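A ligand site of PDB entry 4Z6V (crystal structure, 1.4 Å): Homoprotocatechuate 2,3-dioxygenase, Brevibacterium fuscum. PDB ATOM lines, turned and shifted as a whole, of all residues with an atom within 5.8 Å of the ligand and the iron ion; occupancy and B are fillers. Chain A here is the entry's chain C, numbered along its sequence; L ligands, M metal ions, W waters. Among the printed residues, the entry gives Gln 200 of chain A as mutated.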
ATOM      1  N   HIS A 155     -25.614  -6.495 -14.596  1.00  0.00           N
ATOM      2  CA  HIS A 155     -24.888  -7.290 -15.593  1.00  0.00           C
ATOM      3  C   HIS A 155     -23.782  -6.511 -16.243  1.00  0.00           C
ATOM      4  O   HIS A 155     -23.679  -5.278 -16.093  1.00  0.00           O
ATOM      5  CB  HIS A 155     -25.849  -7.873 -16.658  1.00  0.00           C
ATOM      6  CG  HIS A 155     -26.524  -6.859 -17.544  1.00  0.00           C
ATOM      7  ND1 HIS A 155     -27.788  -6.379 -17.281  1.00  0.00           N
ATOM      8  CD2 HIS A 155     -26.154  -6.311 -18.714  1.00  0.00           C
ATOM      9  CE1 HIS A 155     -28.175  -5.583 -18.277  1.00  0.00           C
ATOM     10  NE2 HIS A 155     -27.186  -5.517 -19.150  1.00  0.00           N
ATOM     11  N   PHE A 156     -22.941  -7.244 -16.968  1.00  0.00           N
ATOM     12  CA  PHE A 156     -21.994  -6.709 -17.924  1.00  0.00           C
ATOM     13  C   PHE A 156     -22.442  -7.082 -19.332  1.00  0.00           C
ATOM     14  O   PHE A 156     -23.164  -8.069 -19.540  1.00  0.00           O
ATOM     15  CB  PHE A 156     -20.605  -7.303 -17.660  1.00  0.00           C
ATOM     16  CG  PHE A 156     -20.145  -7.288 -16.218  1.00  0.00           C
ATOM     17  CD1 PHE A 156     -20.057  -6.104 -15.480  1.00  0.00           C
ATOM     18  CD2 PHE A 156     -19.760  -8.461 -15.612  1.00  0.00           C
ATOM     19  CE1 PHE A 156     -19.600  -6.125 -14.174  1.00  0.00           C
ATOM     20  CE2 PHE A 156     -19.279  -8.483 -14.300  1.00  0.00           C
ATOM     21  CZ  PHE A 156     -19.215  -7.317 -13.584  1.00  0.00           C
ATOM     22  N   ASN A 157     -21.920  -6.356 -20.320  1.00  0.00           N
ATOM     23  CA  ASN A 157     -22.106  -6.701 -21.722  1.00  0.00           C
ATOM     24  C   ASN A 157     -20.763  -6.508 -22.450  1.00  0.00           C
ATOM     25  O   ASN A 157     -20.166  -5.446 -22.378  1.00  0.00           O
ATOM     26  CB  ASN A 157     -23.230  -5.890 -22.347  1.00  0.00           C
ATOM     27  CG  ASN A 157     -23.568  -6.352 -23.735  1.00  0.00           C
ATOM     28  OD1 ASN A 157     -22.693  -6.389 -24.608  1.00  0.00           O
ATOM     29  ND2 ASN A 157     -24.813  -6.739 -23.951  1.00  0.00           N
ATOM     30  N   ILE A 181     -30.046 -13.431 -30.529  1.00  0.00           N
ATOM     31  CA  ILE A 181     -30.461 -12.848 -31.810  1.00  0.00           C
ATOM     32  C   ILE A 181     -29.693 -13.575 -32.922  1.00  0.00           C
ATOM     33  O   ILE A 181     -28.469 -13.630 -32.889  1.00  0.00           O
ATOM     34  CB  ILE A 181     -30.194 -11.320 -31.868  1.00  0.00           C
ATOM     35  CG1 ILE A 181     -31.005 -10.559 -30.814  1.00  0.00           C
ATOM     36  CG2 ILE A 181     -30.477 -10.765 -33.254  1.00  0.00           C
ATOM     37  CD1 ILE A 181     -30.684  -9.082 -30.685  1.00  0.00           C
ATOM     38  N   TRP A 192     -27.343 -13.659 -24.417  1.00  0.00           N
ATOM     39  CA  TRP A 192     -27.458 -13.215 -23.032  1.00  0.00           C
ATOM     40  C   TRP A 192     -27.427 -14.432 -22.148  1.00  0.00           C
ATOM     41  O   TRP A 192     -28.050 -15.431 -22.492  1.00  0.00           O
ATOM     42  CB  TRP A 192     -28.778 -12.478 -22.825  1.00  0.00           C
ATOM     43  CG  TRP A 192     -28.802 -11.091 -23.410  1.00  0.00           C
ATOM     44  CD1 TRP A 192     -28.693  -9.943 -22.706  1.00  0.00           C
ATOM     45  CD2 TRP A 192     -28.983 -10.711 -24.788  1.00  0.00           C
ATOM     46  NE1 TRP A 192     -28.764  -8.855 -23.536  1.00  0.00           N
ATOM     47  CE2 TRP A 192     -28.962  -9.297 -24.826  1.00  0.00           C
ATOM     48  CE3 TRP A 192     -29.185 -11.423 -25.985  1.00  0.00           C
ATOM     49  CZ2 TRP A 192     -29.115  -8.586 -26.011  1.00  0.00           C
ATOM     50  CZ3 TRP A 192     -29.324 -10.718 -27.163  1.00  0.00           C
ATOM     51  CH2 TRP A 192     -29.317  -9.300 -27.166  1.00  0.00           C
ATOM     52  N   GLN A 200     -29.580 -12.099 -17.240  1.00  0.00           N
ATOM     53  CA  GLN A 200     -28.167 -12.042 -17.566  1.00  0.00           C
ATOM     54  C   GLN A 200     -27.303 -11.669 -16.354  1.00  0.00           C
ATOM     55  O   GLN A 200     -27.708 -10.871 -15.515  1.00  0.00           O
ATOM     56  CB  GLN A 200     -27.926 -11.034 -18.702  1.00  0.00           C
ATOM     57  CG  GLN A 200     -28.610  -9.700 -18.391  1.00  0.00           C
ATOM     58  CD  GLN A 200     -28.476  -8.747 -19.546  1.00  0.00           C
ATOM     59  OE1 GLN A 200     -27.427  -8.663 -20.150  1.00  0.00           O
ATOM     60  NE2 GLN A 200     -29.536  -8.002 -19.832  1.00  0.00           N
ATOM     61  N   HIS A 214     -21.019  -2.335 -21.972  1.00  0.00           N
ATOM     62  CA  HIS A 214     -21.587  -1.553 -20.858  1.00  0.00           C
ATOM     63  C   HIS A 214     -21.574  -2.320 -19.550  1.00  0.00           C
ATOM     64  O   HIS A 214     -21.388  -3.551 -19.516  1.00  0.00           O
ATOM     65  CB  HIS A 214     -23.023  -1.056 -21.162  1.00  0.00           C
ATOM     66  CG  HIS A 214     -24.014  -2.119 -21.484  1.00  0.00           C
ATOM     67  ND1 HIS A 214     -24.268  -2.525 -22.765  1.00  0.00           N
ATOM     68  CD2 HIS A 214     -24.892  -2.791 -20.705  1.00  0.00           C
ATOM     69  CE1 HIS A 214     -25.222  -3.430 -22.775  1.00  0.00           C
ATOM     70  NE2 HIS A 214     -25.621  -3.610 -21.528  1.00  0.00           N
ATOM     71  N   ALA A 216     -24.350  -2.541 -16.349  1.00  0.00           N
ATOM     72  CA  ALA A 216     -25.782  -2.228 -16.095  1.00  0.00           C
ATOM     73  C   ALA A 216     -26.110  -2.271 -14.621  1.00  0.00           C
ATOM     74  O   ALA A 216     -25.769  -3.249 -13.922  1.00  0.00           O
ATOM     75  CB  ALA A 216     -26.684  -3.206 -16.828  1.00  0.00           C
ATOM     76  N   ARG A 243     -28.996   6.355 -25.877  1.00  0.00           N
ATOM     77  CA  ARG A 243     -30.069   5.532 -26.413  1.00  0.00           C
ATOM     78  C   ARG A 243     -31.098   5.317 -25.333  1.00  0.00           C
ATOM     79  O   ARG A 243     -30.751   5.047 -24.183  1.00  0.00           O
ATOM     80  CB  ARG A 243     -29.513   4.198 -26.922  1.00  0.00           C
ATOM     81  CG  ARG A 243     -30.580   3.185 -27.333  1.00  0.00           C
ATOM     82  CD  ARG A 243     -30.052   1.900 -27.950  1.00  0.00           C
ATOM     83  NE  ARG A 243     -31.169   0.955 -27.976  1.00  0.00           N
ATOM     84  CZ  ARG A 243     -31.136  -0.349 -27.727  1.00  0.00           C
ATOM     85  NH1 ARG A 243     -29.995  -1.033 -27.542  1.00  0.00           N
ATOM     86  NH2 ARG A 243     -32.281  -1.006 -27.656  1.00  0.00           N
ATOM     87  N   HIS A 248     -36.911  -2.948 -23.849  1.00  0.00           N
ATOM     88  CA  HIS A 248     -36.201  -3.931 -24.664  1.00  0.00           C
ATOM     89  C   HIS A 248     -37.182  -5.011 -25.150  1.00  0.00           C
ATOM     90  O   HIS A 248     -38.127  -5.352 -24.446  1.00  0.00           O
ATOM     91  CB  HIS A 248     -35.125  -4.619 -23.859  1.00  0.00           C
ATOM     92  CG  HIS A 248     -33.869  -3.834 -23.649  1.00  0.00           C
ATOM     93  ND1 HIS A 248     -33.180  -3.216 -24.675  1.00  0.00           N
ATOM     94  CD2 HIS A 248     -33.107  -3.664 -22.540  1.00  0.00           C
ATOM     95  CE1 HIS A 248     -32.064  -2.686 -24.198  1.00  0.00           C
ATOM     96  NE2 HIS A 248     -31.991  -2.960 -22.909  1.00  0.00           N
ATOM     97  N   GLY A 249     -36.909  -5.567 -26.320  1.00  0.00           N
ATOM     98  CA  GLY A 249     -37.528  -6.831 -26.729  1.00  0.00           C
ATOM     99  C   GLY A 249     -36.874  -7.967 -25.968  1.00  0.00           C
ATOM    100  O   GLY A 249     -37.432  -8.532 -25.013  1.00  0.00           O
ATOM    101  N   VAL A 250     -35.651  -8.300 -26.361  1.00  0.00           N
ATOM    102  CA  VAL A 250     -34.799  -9.159 -25.546  1.00  0.00           C
ATOM    103  C   VAL A 250     -34.764  -8.635 -24.110  1.00  0.00           C
ATOM    104  O   VAL A 250     -34.455  -7.476 -23.868  1.00  0.00           O
ATOM    105  CB  VAL A 250     -33.354  -9.199 -26.083  1.00  0.00           C
ATOM    106  CG1 VAL A 250     -32.424  -9.913 -25.113  1.00  0.00           C
ATOM    107  CG2 VAL A 250     -33.284  -9.844 -27.454  1.00  0.00           C
ATOM    108  N   SER A 251     -35.082  -9.513 -23.178  1.00  0.00           N
ATOM    109  CA  SER A 251     -35.099  -9.275 -21.709  1.00  0.00           C
ATOM    110  C   SER A 251     -36.387  -8.672 -21.166  1.00  0.00           C
ATOM    111  O   SER A 251     -36.646  -8.815 -19.964  1.00  0.00           O
ATOM    112  CB  SER A 251     -33.920  -8.434 -21.186  1.00  0.00           C
ATOM    113  OG  SER A 251     -34.175  -7.046 -21.322  1.00  0.00           O
ATOM    114  N   TYR A 257     -29.425   3.980 -21.864  1.00  0.00           N
ATOM    115  CA  TYR A 257     -27.954   4.018 -21.953  1.00  0.00           C
ATOM    116  C   TYR A 257     -27.424   5.451 -21.902  1.00  0.00           C
ATOM    117  O   TYR A 257     -27.848   6.333 -22.667  1.00  0.00           O
ATOM    118  CB  TYR A 257     -27.432   3.354 -23.226  1.00  0.00           C
ATOM    119  CG  TYR A 257     -27.851   1.926 -23.377  1.00  0.00           C
ATOM    120  CD1 TYR A 257     -29.021   1.606 -24.040  1.00  0.00           C
ATOM    121  CD2 TYR A 257     -27.075   0.877 -22.886  1.00  0.00           C
ATOM    122  CE1 TYR A 257     -29.421   0.306 -24.211  1.00  0.00           C
ATOM    123  CE2 TYR A 257     -27.462  -0.444 -23.045  1.00  0.00           C
ATOM    124  CZ  TYR A 257     -28.651  -0.714 -23.711  1.00  0.00           C
ATOM    125  OH  TYR A 257     -29.098  -1.972 -23.936  1.00  0.00           O
ATOM    126  N   GLU A 267     -25.708   1.181 -18.591  1.00  0.00           N
ATOM    127  CA  GLU A 267     -27.129   0.918 -18.795  1.00  0.00           C
ATOM    128  C   GLU A 267     -27.844   1.001 -17.442  1.00  0.00           C
ATOM    129  O   GLU A 267     -27.326   0.556 -16.402  1.00  0.00           O
ATOM    130  CB  GLU A 267     -27.377  -0.468 -19.405  1.00  0.00           C
ATOM    131  CG  GLU A 267     -28.814  -0.706 -19.831  1.00  0.00           C
ATOM    132  CD  GLU A 267     -29.082  -2.077 -20.413  1.00  0.00           C
ATOM    133  OE1 GLU A 267     -28.162  -2.939 -20.325  1.00  0.00           O
ATOM    134  OE2 GLU A 267     -30.168  -2.243 -21.003  1.00  0.00           O
ATOM    135  N   TYR A 269     -31.547  -0.282 -15.951  1.00  0.00           N
ATOM    136  CA  TYR A 269     -32.320  -1.460 -16.373  1.00  0.00           C
ATOM    137  C   TYR A 269     -33.283  -1.846 -15.257  1.00  0.00           C
ATOM    138  O   TYR A 269     -32.917  -1.811 -14.078  1.00  0.00           O
ATOM    139  CB  TYR A 269     -31.305  -2.547 -16.606  1.00  0.00           C
ATOM    140  CG  TYR A 269     -31.685  -3.924 -17.055  1.00  0.00           C
ATOM    141  CD1 TYR A 269     -31.586  -4.300 -18.387  1.00  0.00           C
ATOM    142  CD2 TYR A 269     -31.987  -4.907 -16.112  1.00  0.00           C
ATOM    143  CE1 TYR A 269     -31.807  -5.611 -18.770  1.00  0.00           C
ATOM    144  CE2 TYR A 269     -32.182  -6.224 -16.502  1.00  0.00           C
ATOM    145  CZ  TYR A 269     -32.105  -6.562 -17.840  1.00  0.00           C
ATOM    146  OH  TYR A 269     -32.297  -7.863 -18.268  1.00  0.00           O
ATOM    147  N   ARG A 292     -36.937  -6.149 -31.581  1.00  0.00           N
ATOM    148  CA  ARG A 292     -36.079  -7.039 -30.806  1.00  0.00           C
ATOM    149  C   ARG A 292     -35.232  -6.281 -29.768  1.00  0.00           C
ATOM    150  O   ARG A 292     -34.949  -6.819 -28.714  1.00  0.00           O
ATOM    151  CB  ARG A 292     -35.176  -7.858 -31.724  1.00  0.00           C
ATOM    152  CG  ARG A 292     -33.985  -7.086 -32.254  1.00  0.00           C
ATOM    153  CD  ARG A 292     -33.252  -7.736 -33.433  1.00  0.00           C
ATOM    154  NE  ARG A 292     -32.162  -6.847 -33.818  1.00  0.00           N
ATOM    155  CZ  ARG A 292     -32.311  -5.682 -34.455  1.00  0.00           C
ATOM    156  NH1 ARG A 292     -33.499  -5.276 -34.879  1.00  0.00           N
ATOM    157  NH2 ARG A 292     -31.267  -4.914 -34.688  1.00  0.00           N
ATOM    158  N   ARG A 293     -34.774  -5.083 -30.108  1.00  0.00           N
ATOM    159  CA  ARG A 293     -33.903  -4.309 -29.237  1.00  0.00           C
ATOM    160  C   ARG A 293     -34.650  -3.202 -28.517  1.00  0.00           C
ATOM    161  O   ARG A 293     -34.502  -3.031 -27.295  1.00  0.00           O
ATOM    162  CB  ARG A 293     -32.703  -3.790 -30.018  1.00  0.00           C
ATOM    163  CG  ARG A 293     -31.684  -4.904 -30.302  1.00  0.00           C
ATOM    164  CD  ARG A 293     -30.310  -4.324 -30.558  1.00  0.00           C
ATOM    165  NE  ARG A 293     -29.314  -5.359 -30.763  1.00  0.00           N
ATOM    166  CZ  ARG A 293     -28.592  -5.975 -29.826  1.00  0.00           C
ATOM    167  NH1 ARG A 293     -28.744  -5.706 -28.547  1.00  0.00           N
ATOM    168  NH2 ARG A 293     -27.684  -6.879 -30.190  1.00  0.00           N
ATOM    169  N   ASP A 294     -35.455  -2.462 -29.269  1.00  0.00           N
ATOM    170  CA  ASP A 294     -36.428  -1.564 -28.696  1.00  0.00           C
ATOM    171  C   ASP A 294     -37.779  -2.070 -29.148  1.00  0.00           C
ATOM    172  O   ASP A 294     -38.103  -2.058 -30.353  1.00  0.00           O
ATOM    173  CB  ASP A 294     -36.214  -0.128 -29.139  1.00  0.00           C
ATOM    174  CG  ASP A 294     -37.111   0.840 -28.380  1.00  0.00           C
ATOM    175  OD1 ASP A 294     -36.713   1.237 -27.241  1.00  0.00           O
ATOM    176  OD2 ASP A 294     -38.208   1.189 -28.898  1.00  0.00           O
ATOM    177  N   TRP A 304     -24.190   2.986 -30.784  1.00  0.00           N
ATOM    178  CA  TRP A 304     -24.481   1.863 -29.872  1.00  0.00           C
ATOM    179  C   TRP A 304     -23.870   0.573 -30.410  1.00  0.00           C
ATOM    180  O   TRP A 304     -23.406  -0.276 -29.643  1.00  0.00           O
ATOM    181  CB  TRP A 304     -25.983   1.699 -29.656  1.00  0.00           C
ATOM    182  CG  TRP A 304     -26.320   0.877 -28.452  1.00  0.00           C
ATOM    183  CD1 TRP A 304     -26.492   1.338 -27.200  1.00  0.00           C
ATOM    184  CD2 TRP A 304     -26.465  -0.561 -28.379  1.00  0.00           C
ATOM    185  NE1 TRP A 304     -26.764   0.321 -26.345  1.00  0.00           N
ATOM    186  CE2 TRP A 304     -26.768  -0.868 -27.036  1.00  0.00           C
ATOM    187  CE3 TRP A 304     -26.392  -1.605 -29.305  1.00  0.00           C
ATOM    188  CZ2 TRP A 304     -26.970  -2.165 -26.588  1.00  0.00           C
ATOM    189  CZ3 TRP A 304     -26.555  -2.891 -28.860  1.00  0.00           C
ATOM    190  CH2 TRP A 304     -26.864  -3.168 -27.508  1.00  0.00           C
HETATM  191  C1  LIG L   1     -29.846  -5.683 -22.548  1.00  0.00           C
HETATM  192  C2  LIG L   1     -29.093  -4.877 -23.553  1.00  0.00           C
HETATM  193  C3  LIG L   1     -29.549  -4.818 -24.860  1.00  0.00           C
HETATM  194  C4  LIG L   1     -30.762  -5.459 -25.194  1.00  0.00           C
HETATM  195  C5  LIG L   1     -31.472  -6.221 -24.237  1.00  0.00           C
HETATM  196  C6  LIG L   1     -30.997  -6.371 -22.917  1.00  0.00           C
HETATM  197  O1  LIG L   1     -29.337  -5.674 -21.306  1.00  0.00           O
HETATM  198  O2  LIG L   1     -27.992  -4.202 -23.127  1.00  0.00           O
HETATM  199  N1  LIG L   1     -31.308  -5.207 -26.442  1.00  0.00           N
HETATM  200  O3  LIG L   1     -32.499  -5.706 -26.698  1.00  0.00           O
HETATM  201  O4  LIG L   1     -30.811  -3.959 -27.142  1.00  0.00           O
HETATM  202 FE    FE M   1     -27.535  -4.654 -21.164  1.00  0.00          FE
HETATM  203  O   HOH W   1     -26.752  -6.598 -21.966  1.00  0.00           O
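Within 4 Å of the iron ion: His 155, His 214 and Glu 267.
The iron ion is bound by OE1 of Glu 267 (2.0 Å), O2 of the ligand (2.1 Å), O1 of the ligand (2.1 Å), NE2 of His 214 (2.2 Å), NE2 of His 155 (2.2 Å) and water W1 (2.2 Å).
O of Arg 292 lies close to O3 of the ligand (3.4 Å). Residues that only touch the ligand: Trp 192 (3.4 Å), Val 250 (3.3 Å), Ser 251 (3.6 Å) and Tyr 269 (3.5 Å). Hydrophobic or aromatic side chains within 4 Å of the ligand: His 155, Trp 192, His 214, His 248, Val 250, Tyr 257 and Tyr 269. Within 4 Å of the ligand: His 155, Trp 192, Gln 200, His 214, Arg 243, His 248, Val 250, Ser 251, Tyr 257, Glu 267, Tyr 269, Arg 292 and Arg 293.
O of Arg 292 is in hydrogen-bond range of N of Val 250 (2.9 Å). ND1 of His 248 is in hydrogen-bond range of O of Arg 293 (2.9 Å). NE2 of Gln 200 lies close to ND1 of His 155, 3.5 Å away. O of His 155 sits at hydrogen-bond distance from N of Ala 216 (2.8 Å). NE2 of His 248 lies close to OH of Tyr 257 (3.2 Å). OH of Tyr 257 is in hydrogen-bond range of OE2 of Glu 267 (3.1 Å). The guanidinium group (NH2) of Arg 243 sits at hydrogen-bond distance from the backbone carbonyl oxygen (O) of Arg 293, 3.0 Å away. The backbone NH (N) of Tyr 257 lies within hydrogen-bond range of the backbone carbonyl oxygen (O) of Arg 243, 2.9 Å away.
Water W1 lies within hydrogen-bond range of the side-chain amide nitrogen of Asn 157 (2.8 Å), the side-chain amide oxygen of Gln 200 (2.8 Å) and the indole nitrogen of Trp 192 (3.4 Å).
An oxygen (O3) of the ligand lies within hydrogen-bond range of a ring nitrogen (ND1) of His 248, 3.3 Å away. O4 of the ligand lies within hydrogen-bond range of NH1 of Arg 293, 3.0 Å away. The guanidinium group of Arg 243 sits at hydrogen-bond distance from an oxygen (O4) of the ligand (3.1 Å). The side-chain amide nitrogen of Gln 200 lies close to an oxygen (O1) of the ligand (2.8 Å). O2 of the ligand lies close to OH of Tyr 257, at 2.6 Å.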
